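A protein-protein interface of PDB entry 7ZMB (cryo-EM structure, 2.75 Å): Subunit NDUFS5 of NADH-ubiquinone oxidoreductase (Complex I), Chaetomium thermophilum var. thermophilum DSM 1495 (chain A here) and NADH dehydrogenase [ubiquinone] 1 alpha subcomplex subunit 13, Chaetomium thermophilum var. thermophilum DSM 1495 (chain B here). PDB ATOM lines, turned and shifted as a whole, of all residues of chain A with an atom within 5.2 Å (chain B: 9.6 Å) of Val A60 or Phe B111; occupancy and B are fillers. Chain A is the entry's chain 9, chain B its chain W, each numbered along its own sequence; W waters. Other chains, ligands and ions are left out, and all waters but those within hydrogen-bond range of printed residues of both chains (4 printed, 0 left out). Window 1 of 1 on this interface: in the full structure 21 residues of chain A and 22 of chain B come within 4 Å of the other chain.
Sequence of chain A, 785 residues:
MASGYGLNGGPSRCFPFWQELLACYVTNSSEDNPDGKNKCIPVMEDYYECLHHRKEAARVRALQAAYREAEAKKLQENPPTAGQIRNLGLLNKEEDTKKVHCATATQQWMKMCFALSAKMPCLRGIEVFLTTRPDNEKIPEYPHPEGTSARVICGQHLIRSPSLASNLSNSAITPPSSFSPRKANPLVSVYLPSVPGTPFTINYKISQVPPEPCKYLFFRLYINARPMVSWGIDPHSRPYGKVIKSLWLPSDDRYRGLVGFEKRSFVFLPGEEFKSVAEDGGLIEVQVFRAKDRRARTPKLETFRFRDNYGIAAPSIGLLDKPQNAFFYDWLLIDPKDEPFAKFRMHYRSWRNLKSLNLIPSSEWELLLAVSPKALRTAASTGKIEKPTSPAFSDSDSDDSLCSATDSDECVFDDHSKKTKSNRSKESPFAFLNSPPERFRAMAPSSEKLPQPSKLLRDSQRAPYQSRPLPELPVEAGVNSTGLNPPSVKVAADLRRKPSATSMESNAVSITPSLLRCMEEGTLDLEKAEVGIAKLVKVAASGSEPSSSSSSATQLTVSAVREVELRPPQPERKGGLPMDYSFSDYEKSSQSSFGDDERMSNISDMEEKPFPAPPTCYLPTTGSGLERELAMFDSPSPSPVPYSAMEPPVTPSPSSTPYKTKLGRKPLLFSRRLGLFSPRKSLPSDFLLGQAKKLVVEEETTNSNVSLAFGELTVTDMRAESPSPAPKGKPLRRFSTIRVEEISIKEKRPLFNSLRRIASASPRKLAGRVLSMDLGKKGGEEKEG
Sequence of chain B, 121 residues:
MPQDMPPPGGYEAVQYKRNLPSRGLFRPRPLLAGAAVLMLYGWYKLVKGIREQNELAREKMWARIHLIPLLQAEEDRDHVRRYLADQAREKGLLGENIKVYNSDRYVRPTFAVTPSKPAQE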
ATOM      1  N   HIS A  53       2.490 -19.508  -4.122  1.00  0.00           N
ATOM      2  CA  HIS A  53       3.775 -19.868  -4.788  1.00  0.00           C
ATOM      3  C   HIS A  53       3.618 -20.793  -6.007  1.00  0.00           C
ATOM      4  O   HIS A  53       4.625 -21.411  -6.360  1.00  0.00           O
ATOM      5  CB  HIS A  53       4.807 -20.432  -3.798  1.00  0.00           C
ATOM      6  CG  HIS A  53       4.988 -19.638  -2.552  1.00  0.00           C
ATOM      7  ND1 HIS A  53       5.642 -18.427  -2.537  1.00  0.00           N
ATOM      8  CD2 HIS A  53       4.626 -19.892  -1.278  1.00  0.00           C
ATOM      9  CE1 HIS A  53       5.662 -17.960  -1.308  1.00  0.00           C
ATOM     10  NE2 HIS A  53       5.047 -18.840  -0.519  1.00  0.00           N
ATOM     11  N   GLU A  56       6.080 -19.829  -8.945  1.00  0.00           N
ATOM     12  CA  GLU A  56       7.510 -20.015  -8.566  1.00  0.00           C
ATOM     13  C   GLU A  56       7.753 -21.498  -8.367  1.00  0.00           C
ATOM     14  O   GLU A  56       8.902 -21.936  -8.482  1.00  0.00           O
ATOM     15  CB  GLU A  56       7.867 -19.168  -7.349  1.00  0.00           C
ATOM     16  CG  GLU A  56       9.227 -19.418  -6.756  1.00  0.00           C
ATOM     17  CD  GLU A  56       9.302 -18.890  -5.337  1.00  0.00           C
ATOM     18  OE1 GLU A  56       8.249 -18.522  -4.791  1.00  0.00           O
ATOM     19  OE2 GLU A  56      10.406 -18.843  -4.792  1.00  0.00           O
ATOM     20  N   ALA A  57       6.670 -22.239  -8.211  1.00  0.00           N
ATOM     21  CA  ALA A  57       6.788 -23.694  -8.053  1.00  0.00           C
ATOM     22  C   ALA A  57       6.899 -24.210  -9.470  1.00  0.00           C
ATOM     23  O   ALA A  57       7.610 -25.185  -9.695  1.00  0.00           O
ATOM     24  CB  ALA A  57       5.560 -24.239  -7.380  1.00  0.00           C
ATOM     25  N   ALA A  58       6.263 -23.498 -10.390  1.00  0.00           N
ATOM     26  CA  ALA A  58       6.244 -23.995 -11.782  1.00  0.00           C
ATOM     27  C   ALA A  58       7.577 -23.692 -12.461  1.00  0.00           C
ATOM     28  O   ALA A  58       8.039 -24.533 -13.228  1.00  0.00           O
ATOM     29  CB  ALA A  58       5.076 -23.400 -12.503  1.00  0.00           C
ATOM     30  N   ARG A  59       8.163 -22.530 -12.180  1.00  0.00           N
ATOM     31  CA  ARG A  59       9.476 -22.164 -12.748  1.00  0.00           C
ATOM     32  C   ARG A  59      10.557 -23.112 -12.248  1.00  0.00           C
ATOM     33  O   ARG A  59      11.330 -23.606 -13.081  1.00  0.00           O
ATOM     34  CB  ARG A  59       9.834 -20.752 -12.290  1.00  0.00           C
ATOM     35  CG  ARG A  59      11.201 -20.269 -12.739  1.00  0.00           C
ATOM     36  CD  ARG A  59      11.537 -18.947 -12.081  1.00  0.00           C
ATOM     37  NE  ARG A  59      12.960 -18.667 -12.145  1.00  0.00           N
ATOM     38  CZ  ARG A  59      13.856 -19.156 -11.300  1.00  0.00           C
ATOM     39  NH1 ARG A  59      13.478 -19.955 -10.318  1.00  0.00           N
ATOM     40  NH2 ARG A  59      15.131 -18.840 -11.440  1.00  0.00           N
ATOM     41  N   VAL A  60      10.574 -23.395 -10.950  1.00  0.00           N
ATOM     42  CA  VAL A  60      11.659 -24.239 -10.385  1.00  0.00           C
ATOM     43  C   VAL A  60      11.503 -25.656 -10.928  1.00  0.00           C
ATOM     44  O   VAL A  60      12.525 -26.278 -11.172  1.00  0.00           O
ATOM     45  CB  VAL A  60      11.715 -24.164  -8.847  1.00  0.00           C
ATOM     46  CG1 VAL A  60      12.691 -25.162  -8.248  1.00  0.00           C
ATOM     47  CG2 VAL A  60      12.051 -22.755  -8.386  1.00  0.00           C
ATOM     48  N   ARG A  61      10.281 -26.105 -11.206  1.00  0.00           N
ATOM     49  CA  ARG A  61      10.129 -27.443 -11.772  1.00  0.00           C
ATOM     50  C   ARG A  61      10.746 -27.524 -13.160  1.00  0.00           C
ATOM     51  O   ARG A  61      11.448 -28.487 -13.483  1.00  0.00           O
ATOM     52  CB  ARG A  61       8.653 -27.833 -11.826  1.00  0.00           C
ATOM     53  CG  ARG A  61       8.030 -28.017 -10.481  1.00  0.00           C
ATOM     54  CD  ARG A  61       6.579 -28.431 -10.573  1.00  0.00           C
ATOM     55  NE  ARG A  61       5.971 -28.513  -9.251  1.00  0.00           N
ATOM     56  CZ  ARG A  61       5.975 -29.603  -8.493  1.00  0.00           C
ATOM     57  NH1 ARG A  61       6.553 -30.713  -8.930  1.00  0.00           N
ATOM     58  NH2 ARG A  61       5.397 -29.584  -7.299  1.00  0.00           N
ATOM     59  N   ALA A  62      10.481 -26.523 -13.996  1.00  0.00           N
ATOM     60  CA  ALA A  62      11.057 -26.493 -15.336  1.00  0.00           C
ATOM     61  C   ALA A  62      12.579 -26.439 -15.285  1.00  0.00           C
ATOM     62  O   ALA A  62      13.262 -27.246 -15.923  1.00  0.00           O
ATOM     63  CB  ALA A  62      10.505 -25.296 -16.106  1.00  0.00           C
ATOM     64  N   LEU A  63      13.130 -25.496 -14.523  1.00  0.00           N
ATOM     65  CA  LEU A  63      14.570 -25.294 -14.550  1.00  0.00           C
ATOM     66  C   LEU A  63      15.291 -26.459 -13.887  1.00  0.00           C
ATOM     67  O   LEU A  63      16.380 -26.847 -14.319  1.00  0.00           O
ATOM     68  CB  LEU A  63      14.926 -23.983 -13.856  1.00  0.00           C
ATOM     69  CG  LEU A  63      16.356 -23.422 -13.909  1.00  0.00           C
ATOM     70  CD1 LEU A  63      16.273 -21.921 -13.735  1.00  0.00           C
ATOM     71  CD2 LEU A  63      17.377 -24.027 -12.950  1.00  0.00           C
ATOM     72  N   GLN A  64      14.690 -27.033 -12.846  1.00  0.00           N
ATOM     73  CA  GLN A  64      15.301 -28.150 -12.142  1.00  0.00           C
ATOM     74  C   GLN A  64      15.396 -29.390 -13.021  1.00  0.00           C
ATOM     75  O   GLN A  64      16.365 -30.147 -12.916  1.00  0.00           O
ATOM     76  CB  GLN A  64      14.499 -28.454 -10.884  1.00  0.00           C
ATOM     77  CG  GLN A  64      15.059 -29.526 -10.002  1.00  0.00           C
ATOM     78  CD  GLN A  64      14.219 -29.703  -8.777  1.00  0.00           C
ATOM     79  OE1 GLN A  64      13.197 -29.044  -8.616  1.00  0.00           O
ATOM     80  NE2 GLN A  64      14.633 -30.589  -7.906  1.00  0.00           N
ATOM     81  N   ALA A  65      14.400 -29.631 -13.865  1.00  0.00           N
ATOM     82  CA  ALA A  65      14.498 -30.748 -14.796  1.00  0.00           C
ATOM     83  C   ALA A  65      15.527 -30.449 -15.877  1.00  0.00           C
ATOM     84  O   ALA A  65      16.347 -31.307 -16.224  1.00  0.00           O
ATOM     85  CB  ALA A  65      13.132 -31.046 -15.407  1.00  0.00           C
ATOM     86  N   ARG B  82      23.206 -14.544  -5.712  1.00  0.00           N
ATOM     87  CA  ARG B  82      22.557 -15.809  -6.139  1.00  0.00           C
ATOM     88  C   ARG B  82      21.389 -15.548  -7.074  1.00  0.00           C
ATOM     89  O   ARG B  82      21.093 -16.434  -7.874  1.00  0.00           O
ATOM     90  CB  ARG B  82      22.196 -16.675  -4.927  1.00  0.00           C
ATOM     91  CG  ARG B  82      23.392 -17.018  -4.050  1.00  0.00           C
ATOM     92  CD  ARG B  82      23.137 -17.945  -2.881  1.00  0.00           C
ATOM     93  NE  ARG B  82      22.667 -19.255  -3.297  1.00  0.00           N
ATOM     94  CZ  ARG B  82      22.743 -20.354  -2.559  1.00  0.00           C
ATOM     95  NH1 ARG B  82      22.278 -21.497  -3.031  1.00  0.00           N
ATOM     96  NH2 ARG B  82      23.292 -20.311  -1.360  1.00  0.00           N
ATOM     97  N   ASP B  86      21.091 -17.221 -10.713  1.00  0.00           N
ATOM     98  CA  ASP B  86      19.914 -18.017 -11.163  1.00  0.00           C
ATOM     99  C   ASP B  86      19.351 -17.456 -12.469  1.00  0.00           C
ATOM    100  O   ASP B  86      18.920 -18.246 -13.325  1.00  0.00           O
ATOM    101  CB  ASP B  86      18.862 -18.123 -10.065  1.00  0.00           C
ATOM    102  CG  ASP B  86      18.134 -19.455 -10.064  1.00  0.00           C
ATOM    103  OD1 ASP B  86      18.619 -20.387 -10.737  1.00  0.00           O
ATOM    104  OD2 ASP B  86      17.088 -19.550  -9.391  1.00  0.00           O
ATOM    105  N   GLU B  90      19.065 -19.742 -15.847  1.00  0.00           N
ATOM    106  CA  GLU B  90      17.803 -19.975 -16.530  1.00  0.00           C
ATOM    107  C   GLU B  90      17.878 -19.628 -18.005  1.00  0.00           C
ATOM    108  O   GLU B  90      17.370 -20.379 -18.846  1.00  0.00           O
ATOM    109  CB  GLU B  90      16.699 -19.152 -15.875  1.00  0.00           C
ATOM    110  CG  GLU B  90      15.308 -19.608 -16.192  1.00  0.00           C
ATOM    111  CD  GLU B  90      14.366 -19.351 -15.042  1.00  0.00           C
ATOM    112  OE1 GLU B  90      14.554 -18.332 -14.349  1.00  0.00           O
ATOM    113  OE2 GLU B  90      13.455 -20.173 -14.822  1.00  0.00           O
ATOM    114  N   LEU B  93      19.437 -22.556 -19.682  1.00  0.00           N
ATOM    115  CA  LEU B  93      18.858 -23.891 -19.581  1.00  0.00           C
ATOM    116  C   LEU B  93      17.410 -23.900 -20.041  1.00  0.00           C
ATOM    117  O   LEU B  93      16.960 -24.863 -20.668  1.00  0.00           O
ATOM    118  CB  LEU B  93      18.948 -24.413 -18.148  1.00  0.00           C
ATOM    119  CG  LEU B  93      20.338 -24.715 -17.618  1.00  0.00           C
ATOM    120  CD1 LEU B  93      20.243 -25.244 -16.209  1.00  0.00           C
ATOM    121  CD2 LEU B  93      21.041 -25.702 -18.523  1.00  0.00           C
ATOM    122  N   LEU B  94      16.668 -22.847 -19.722  1.00  0.00           N
ATOM    123  CA  LEU B  94      15.307 -22.714 -20.205  1.00  0.00           C
ATOM    124  C   LEU B  94      15.200 -21.793 -21.412  1.00  0.00           C
ATOM    125  O   LEU B  94      14.093 -21.589 -21.918  1.00  0.00           O
ATOM    126  CB  LEU B  94      14.389 -22.215 -19.079  1.00  0.00           C
ATOM    127  CG  LEU B  94      14.252 -23.142 -17.864  1.00  0.00           C
ATOM    128  CD1 LEU B  94      13.213 -22.622 -16.885  1.00  0.00           C
ATOM    129  CD2 LEU B  94      13.919 -24.557 -18.283  1.00  0.00           C
ATOM    130  N   ILE B  98      11.543 -16.759 -17.277  1.00  0.00           N
ATOM    131  CA  ILE B  98      10.102 -16.611 -17.119  1.00  0.00           C
ATOM    132  C   ILE B  98       9.805 -15.831 -15.846  1.00  0.00           C
ATOM    133  O   ILE B  98      10.614 -15.768 -14.915  1.00  0.00           O
ATOM    134  CB  ILE B  98       9.391 -17.978 -17.132  1.00  0.00           C
ATOM    135  CG1 ILE B  98       9.851 -18.852 -15.972  1.00  0.00           C
ATOM    136  CG2 ILE B  98       9.632 -18.688 -18.455  1.00  0.00           C
ATOM    137  CD1 ILE B  98       9.012 -20.101 -15.818  1.00  0.00           C
ATOM    138  N   LYS B  99       8.656 -15.136 -15.843  1.00  0.00           N
ATOM    139  CA  LYS B  99       8.397 -14.221 -14.698  1.00  0.00           C
ATOM    140  C   LYS B  99       7.442 -14.815 -13.667  1.00  0.00           C
ATOM    141  O   LYS B  99       6.302 -15.140 -14.042  1.00  0.00           O
ATOM    142  CB  LYS B  99       7.868 -12.877 -15.208  1.00  0.00           C
ATOM    143  CG  LYS B  99       8.831 -12.104 -16.097  1.00  0.00           C
ATOM    144  CD  LYS B  99       8.250 -10.816 -16.641  1.00  0.00           C
ATOM    145  CE  LYS B  99       9.233 -10.047 -17.498  1.00  0.00           C
ATOM    146  NZ  LYS B  99       9.734 -10.865 -18.628  1.00  0.00           N
ATOM    147  N   VAL B 100       7.904 -14.941 -12.411  1.00  0.00           N
ATOM    148  CA  VAL B 100       6.971 -15.370 -11.337  1.00  0.00           C
ATOM    149  C   VAL B 100       6.256 -14.124 -10.820  1.00  0.00           C
ATOM    150  O   VAL B 100       5.141 -14.265 -10.296  1.00  0.00           O
ATOM    151  CB  VAL B 100       7.775 -16.062 -10.228  1.00  0.00           C
ATOM    152  CG1 VAL B 100       6.942 -16.377  -9.002  1.00  0.00           C
ATOM    153  CG2 VAL B 100       8.507 -17.290 -10.741  1.00  0.00           C
ATOM    154  N   TYR B 101       6.866 -12.947 -10.958  1.00  0.00           N
ATOM    155  CA  TYR B 101       6.233 -11.738 -10.369  1.00  0.00           C
ATOM    156  C   TYR B 101       6.118 -10.608 -11.378  1.00  0.00           C
ATOM    157  O   TYR B 101       7.097 -10.334 -12.071  1.00  0.00           O
ATOM    158  CB  TYR B 101       6.948 -11.252  -9.108  1.00  0.00           C
ATOM    159  CG  TYR B 101       6.654 -12.049  -7.869  1.00  0.00           C
ATOM    160  CD1 TYR B 101       5.486 -11.846  -7.158  1.00  0.00           C
ATOM    161  CD2 TYR B 101       7.549 -12.994  -7.403  1.00  0.00           C
ATOM    162  CE1 TYR B 101       5.210 -12.567  -6.011  1.00  0.00           C
ATOM    163  CE2 TYR B 101       7.288 -13.727  -6.263  1.00  0.00           C
ATOM    164  CZ  TYR B 101       6.116 -13.509  -5.565  1.00  0.00           C
ATOM    165  OH  TYR B 101       5.853 -14.220  -4.440  1.00  0.00           O
ATOM    166  N   TYR B 106      12.428  -7.527  -5.555  1.00  0.00           N
ATOM    167  CA  TYR B 106      13.111  -8.807  -5.279  1.00  0.00           C
ATOM    168  C   TYR B 106      12.311  -9.581  -4.239  1.00  0.00           C
ATOM    169  O   TYR B 106      11.911  -8.992  -3.221  1.00  0.00           O
ATOM    170  CB  TYR B 106      14.514  -8.578  -4.722  1.00  0.00           C
ATOM    171  CG  TYR B 106      15.171  -9.838  -4.223  1.00  0.00           C
ATOM    172  CD1 TYR B 106      15.498 -10.859  -5.099  1.00  0.00           C
ATOM    173  CD2 TYR B 106      15.435 -10.026  -2.878  1.00  0.00           C
ATOM    174  CE1 TYR B 106      16.081 -12.031  -4.655  1.00  0.00           C
ATOM    175  CE2 TYR B 106      16.022 -11.191  -2.418  1.00  0.00           C
ATOM    176  CZ  TYR B 106      16.347 -12.196  -3.311  1.00  0.00           C
ATOM    177  OH  TYR B 106      16.931 -13.349  -2.879  1.00  0.00           O
ATOM    178  N   VAL B 107      12.110 -10.870  -4.493  1.00  0.00           N
ATOM    179  CA  VAL B 107      11.401 -11.713  -3.504  1.00  0.00           C
ATOM    180  C   VAL B 107      12.355 -12.828  -3.051  1.00  0.00           C
ATOM    181  O   VAL B 107      12.852 -13.563  -3.898  1.00  0.00           O
ATOM    182  CB  VAL B 107      10.072 -12.226  -4.094  1.00  0.00           C
ATOM    183  CG1 VAL B 107       9.257 -13.009  -3.079  1.00  0.00           C
ATOM    184  CG2 VAL B 107       9.237 -11.110  -4.700  1.00  0.00           C
ATOM    185  N   ARG B 108      12.581 -12.959  -1.747  1.00  0.00           N
ATOM    186  CA  ARG B 108      13.432 -14.044  -1.199  1.00  0.00           C
ATOM    187  C   ARG B 108      12.936 -15.423  -1.684  1.00  0.00           C
ATOM    188  O   ARG B 108      11.844 -15.819  -1.239  1.00  0.00           O
ATOM    189  CB  ARG B 108      13.552 -13.860   0.316  1.00  0.00           C
ATOM    190  CG  ARG B 108      14.607 -12.838   0.700  1.00  0.00           C
ATOM    191  CD  ARG B 108      14.393 -12.320   2.099  1.00  0.00           C
ATOM    192  NE  ARG B 108      15.392 -11.336   2.477  1.00  0.00           N
ATOM    193  CZ  ARG B 108      15.234 -10.025   2.364  1.00  0.00           C
ATOM    194  NH1 ARG B 108      16.196  -9.206   2.746  1.00  0.00           N
ATOM    195  NH2 ARG B 108      14.112  -9.535   1.870  1.00  0.00           N
ATOM    196  N   PRO B 109      13.687 -16.206  -2.512  1.00  0.00           N
ATOM    197  CA  PRO B 109      13.197 -17.478  -3.075  1.00  0.00           C
ATOM    198  C   PRO B 109      12.534 -18.472  -2.113  1.00  0.00           C
ATOM    199  O   PRO B 109      13.107 -18.745  -1.094  1.00  0.00           O
ATOM    200  CB  PRO B 109      14.485 -18.128  -3.589  1.00  0.00           C
ATOM    201  CG  PRO B 109      15.382 -16.971  -3.932  1.00  0.00           C
ATOM    202  CD  PRO B 109      15.084 -15.943  -2.865  1.00  0.00           C
ATOM    203  N   THR B 110      11.340 -18.972  -2.440  1.00  0.00           N
ATOM    204  CA  THR B 110      10.701 -20.008  -1.640  1.00  0.00           C
ATOM    205  C   THR B 110      11.157 -21.394  -2.060  1.00  0.00           C
ATOM    206  O   THR B 110      11.274 -22.289  -1.221  1.00  0.00           O
ATOM    207  CB  THR B 110       9.179 -19.897  -1.761  1.00  0.00           C
ATOM    208  OG1 THR B 110       8.750 -18.643  -1.230  1.00  0.00           O
ATOM    209  CG2 THR B 110       8.483 -21.017  -1.016  1.00  0.00           C
ATOM    210  N   PHE B 111      11.432 -21.569  -3.347  1.00  0.00           N
ATOM    211  CA  PHE B 111      11.917 -22.809  -3.916  1.00  0.00           C
ATOM    212  C   PHE B 111      13.262 -22.541  -4.563  1.00  0.00           C
ATOM    213  O   PHE B 111      13.488 -21.466  -5.119  1.00  0.00           O
ATOM    214  CB  PHE B 111      10.946 -23.367  -4.965  1.00  0.00           C
ATOM    215  CG  PHE B 111       9.561 -23.585  -4.454  1.00  0.00           C
ATOM    216  CD1 PHE B 111       9.273 -24.647  -3.617  1.00  0.00           C
ATOM    217  CD2 PHE B 111       8.541 -22.722  -4.807  1.00  0.00           C
ATOM    218  CE1 PHE B 111       8.000 -24.845  -3.151  1.00  0.00           C
ATOM    219  CE2 PHE B 111       7.264 -22.918  -4.342  1.00  0.00           C
ATOM    220  CZ  PHE B 111       6.992 -23.980  -3.510  1.00  0.00           C
ATOM    221  N   ALA B 112      14.152 -23.519  -4.491  1.00  0.00           N
ATOM    222  CA  ALA B 112      15.434 -23.445  -5.166  1.00  0.00           C
ATOM    223  C   ALA B 112      15.652 -24.715  -5.966  1.00  0.00           C
ATOM    224  O   ALA B 112      15.225 -25.799  -5.569  1.00  0.00           O
ATOM    225  CB  ALA B 112      16.591 -23.253  -4.186  1.00  0.00           C
ATOM    226  N   VAL B 113      16.316 -24.562  -7.110  1.00  0.00           N
ATOM    227  CA  VAL B 113      16.785 -25.715  -7.859  1.00  0.00           C
ATOM    228  C   VAL B 113      17.991 -26.317  -7.153  1.00  0.00           C
ATOM    229  O   VAL B 113      18.942 -25.608  -6.799  1.00  0.00           O
ATOM    230  CB  VAL B 113      17.121 -25.317  -9.300  1.00  0.00           C
ATOM    231  CG1 VAL B 113      17.708 -26.487 -10.037  1.00  0.00           C
ATOM    232  CG2 VAL B 113      15.877 -24.838  -9.992  1.00  0.00           C
ATOM    233  N   THR B 114      17.949 -27.619  -6.928  1.00  0.00           N
ATOM    234  CA  THR B 114      19.035 -28.359  -6.316  1.00  0.00           C
ATOM    235  C   THR B 114      19.569 -29.395  -7.292  1.00  0.00           C
ATOM    236  O   THR B 114      18.855 -29.830  -8.202  1.00  0.00           O
ATOM    237  CB  THR B 114      18.577 -29.067  -5.030  1.00  0.00           C
ATOM    238  OG1 THR B 114      17.874 -30.268  -5.365  1.00  0.00           O
ATOM    239  CG2 THR B 114      17.672 -28.175  -4.208  1.00  0.00           C
ATOM    240  N   PRO B 115      20.823 -29.811  -7.138  1.00  0.00           N
ATOM    241  CA  PRO B 115      21.301 -30.978  -7.878  1.00  0.00           C
ATOM    242  C   PRO B 115      20.618 -32.245  -7.397  1.00  0.00           C
ATOM    243  O   PRO B 115      20.070 -32.313  -6.295  1.00  0.00           O
ATOM    244  CB  PRO B 115      22.801 -30.999  -7.576  1.00  0.00           C
ATOM    245  CG  PRO B 115      22.932 -30.266  -6.304  1.00  0.00           C
ATOM    246  CD  PRO B 115      21.897 -29.196  -6.342  1.00  0.00           C
HETATM  247  O   HOH W   1       9.215 -16.375  -2.454  1.00  0.00           O
HETATM  248  O   HOH W   2       6.268 -16.725  -5.121  1.00  0.00           O
HETATM  249  O   HOH W   3      14.231 -28.357  -5.790  1.00  0.00           O
HETATM  250  O   HOH W   4       6.668 -15.239  -2.219  1.00  0.00           O
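Phe B111 touches four residues of chain A.
Of the printed residues of chain B, Ala A57 touches Phe B111 (3.7 Å).
Of chain B, only Leu B94 (3.6 Å) comes within 4 Å of Ala A62.
Of the printed residues of chain A, Ala B112 touches Val A60 (3.7 Å).
Printed residues of chain B within 4 Å of Gln A64: Val B113 (3.6 Å).
Of the printed residues of chain B, Leu A63 touches Glu B90, Leu B94 and Val B113.
Of the printed residues of chain A, Val B100 touches Glu A56 and Arg A59.
Ala A65 touches none of the printed residues of chain B.
Thr B114 touches none of the printed residues of chain A.
The nearest printed residue of chain A that does not touch Phe B111 is Arg A59 (5.4 Å).
The nearest printed residue of chain B that does not touch Gln A64 is Thr B114 (4.1 Å).
OD2 of Asp B86 lies within salt-bridge range of NH2 of Arg A59.
The side-chain carboxylate of Glu B90 lies within salt-bridge range of the guanidinium group of Arg A59.
The side-chain hydroxyl (OG1) of Thr B110 sits close to a ring nitrogen (ND1) of His A53.
The backbone NH (N) of Thr B110 is in hydrogen-bond range of the side-chain carboxylate (OE2) of Glu A56, 2.5 Å away.
OE2 of Glu A56 is in hydrogen-bond range of N of Phe B111, 3.3 Å away.
ND1 of His A53 is in hydrogen-bond range of OE1 of Glu A56, 3.4 Å away.
His A53 touches Phe B111 (CB to CE2, 3.5 Å).
Glu A56 touches Val B100.
Phe B111 touches Ala A57 (CE2 to CB, 3.7 Å).
CB of Arg A59 touches CD1 of Ile B98 (3.7 Å).
CD of Arg A59 touches CG2 of Val B100, 3.7 Å away.
CG2 of Val A60 touches CB of Phe B111 (3.6 Å).
Ala A62 touches Leu B94 (O to CD2, 3.6 Å).
Leu A63 touches Glu B90 (CD1 to CD, 3.5 Å).
Val B113 touches Leu A63.
Val B113 touches Gln A64.
Water W4 lies within hydrogen-bond range of OH of Tyr B101 (2.6 Å) and ND1 of His A53 (3.4 Å).
Water W1 lies within hydrogen-bond range of the side-chain hydroxyl (OG1) of Thr B110, the backbone carbonyl oxygen (O) of Arg B108 and the side-chain carboxylate (OE1) of Glu A56.
Water W2 lies within hydrogen-bond range of the side-chain hydroxyl (OH) of Tyr B101 (2.6 Å), the side-chain carboxylate (OE1) of Glu A56 (2.7 Å) and a ring nitrogen (ND1) of His A53 (3.2 Å).
Water W3 lies within hydrogen-bond range of O of Ala B112 (2.8 Å) and OE1 of Gln A64 (3.1 Å).
Of the 19 printed residues of chain B, 10 touch a printed residue of chain A.
Printed residues of chain B that touch a printed residue of chain A: Asp B86, Glu B90, Leu B94, Ile B98, Val B100, Pro B109, Thr B110, Phe B111, Ala B112 and Val B113.
Hydrophobic or aromatic side chains of chain B within 4 Å of the printed part of chain A: Leu B94, Ile B98, Val B100, Phe B111 and Val B113.
Of the 11 printed residues of chain A, 8 touch a printed residue of chain B.
Hydrophobic or aromatic side chains of chain A within 4 Å of the printed part of chain B: His A53, Ala A57, Val A60, Ala A62 and Leu A63.
Among the printed residues, 19 pairs touch across the chains.
Among the printed residues, Asp or Glu carboxylates within 4 Å of a Lys or Arg side-chain nitrogen of the other chain: Arg A59 with Asp B86 (2.9 Å) and Arg A59 with Glu B90 (2.7 Å).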
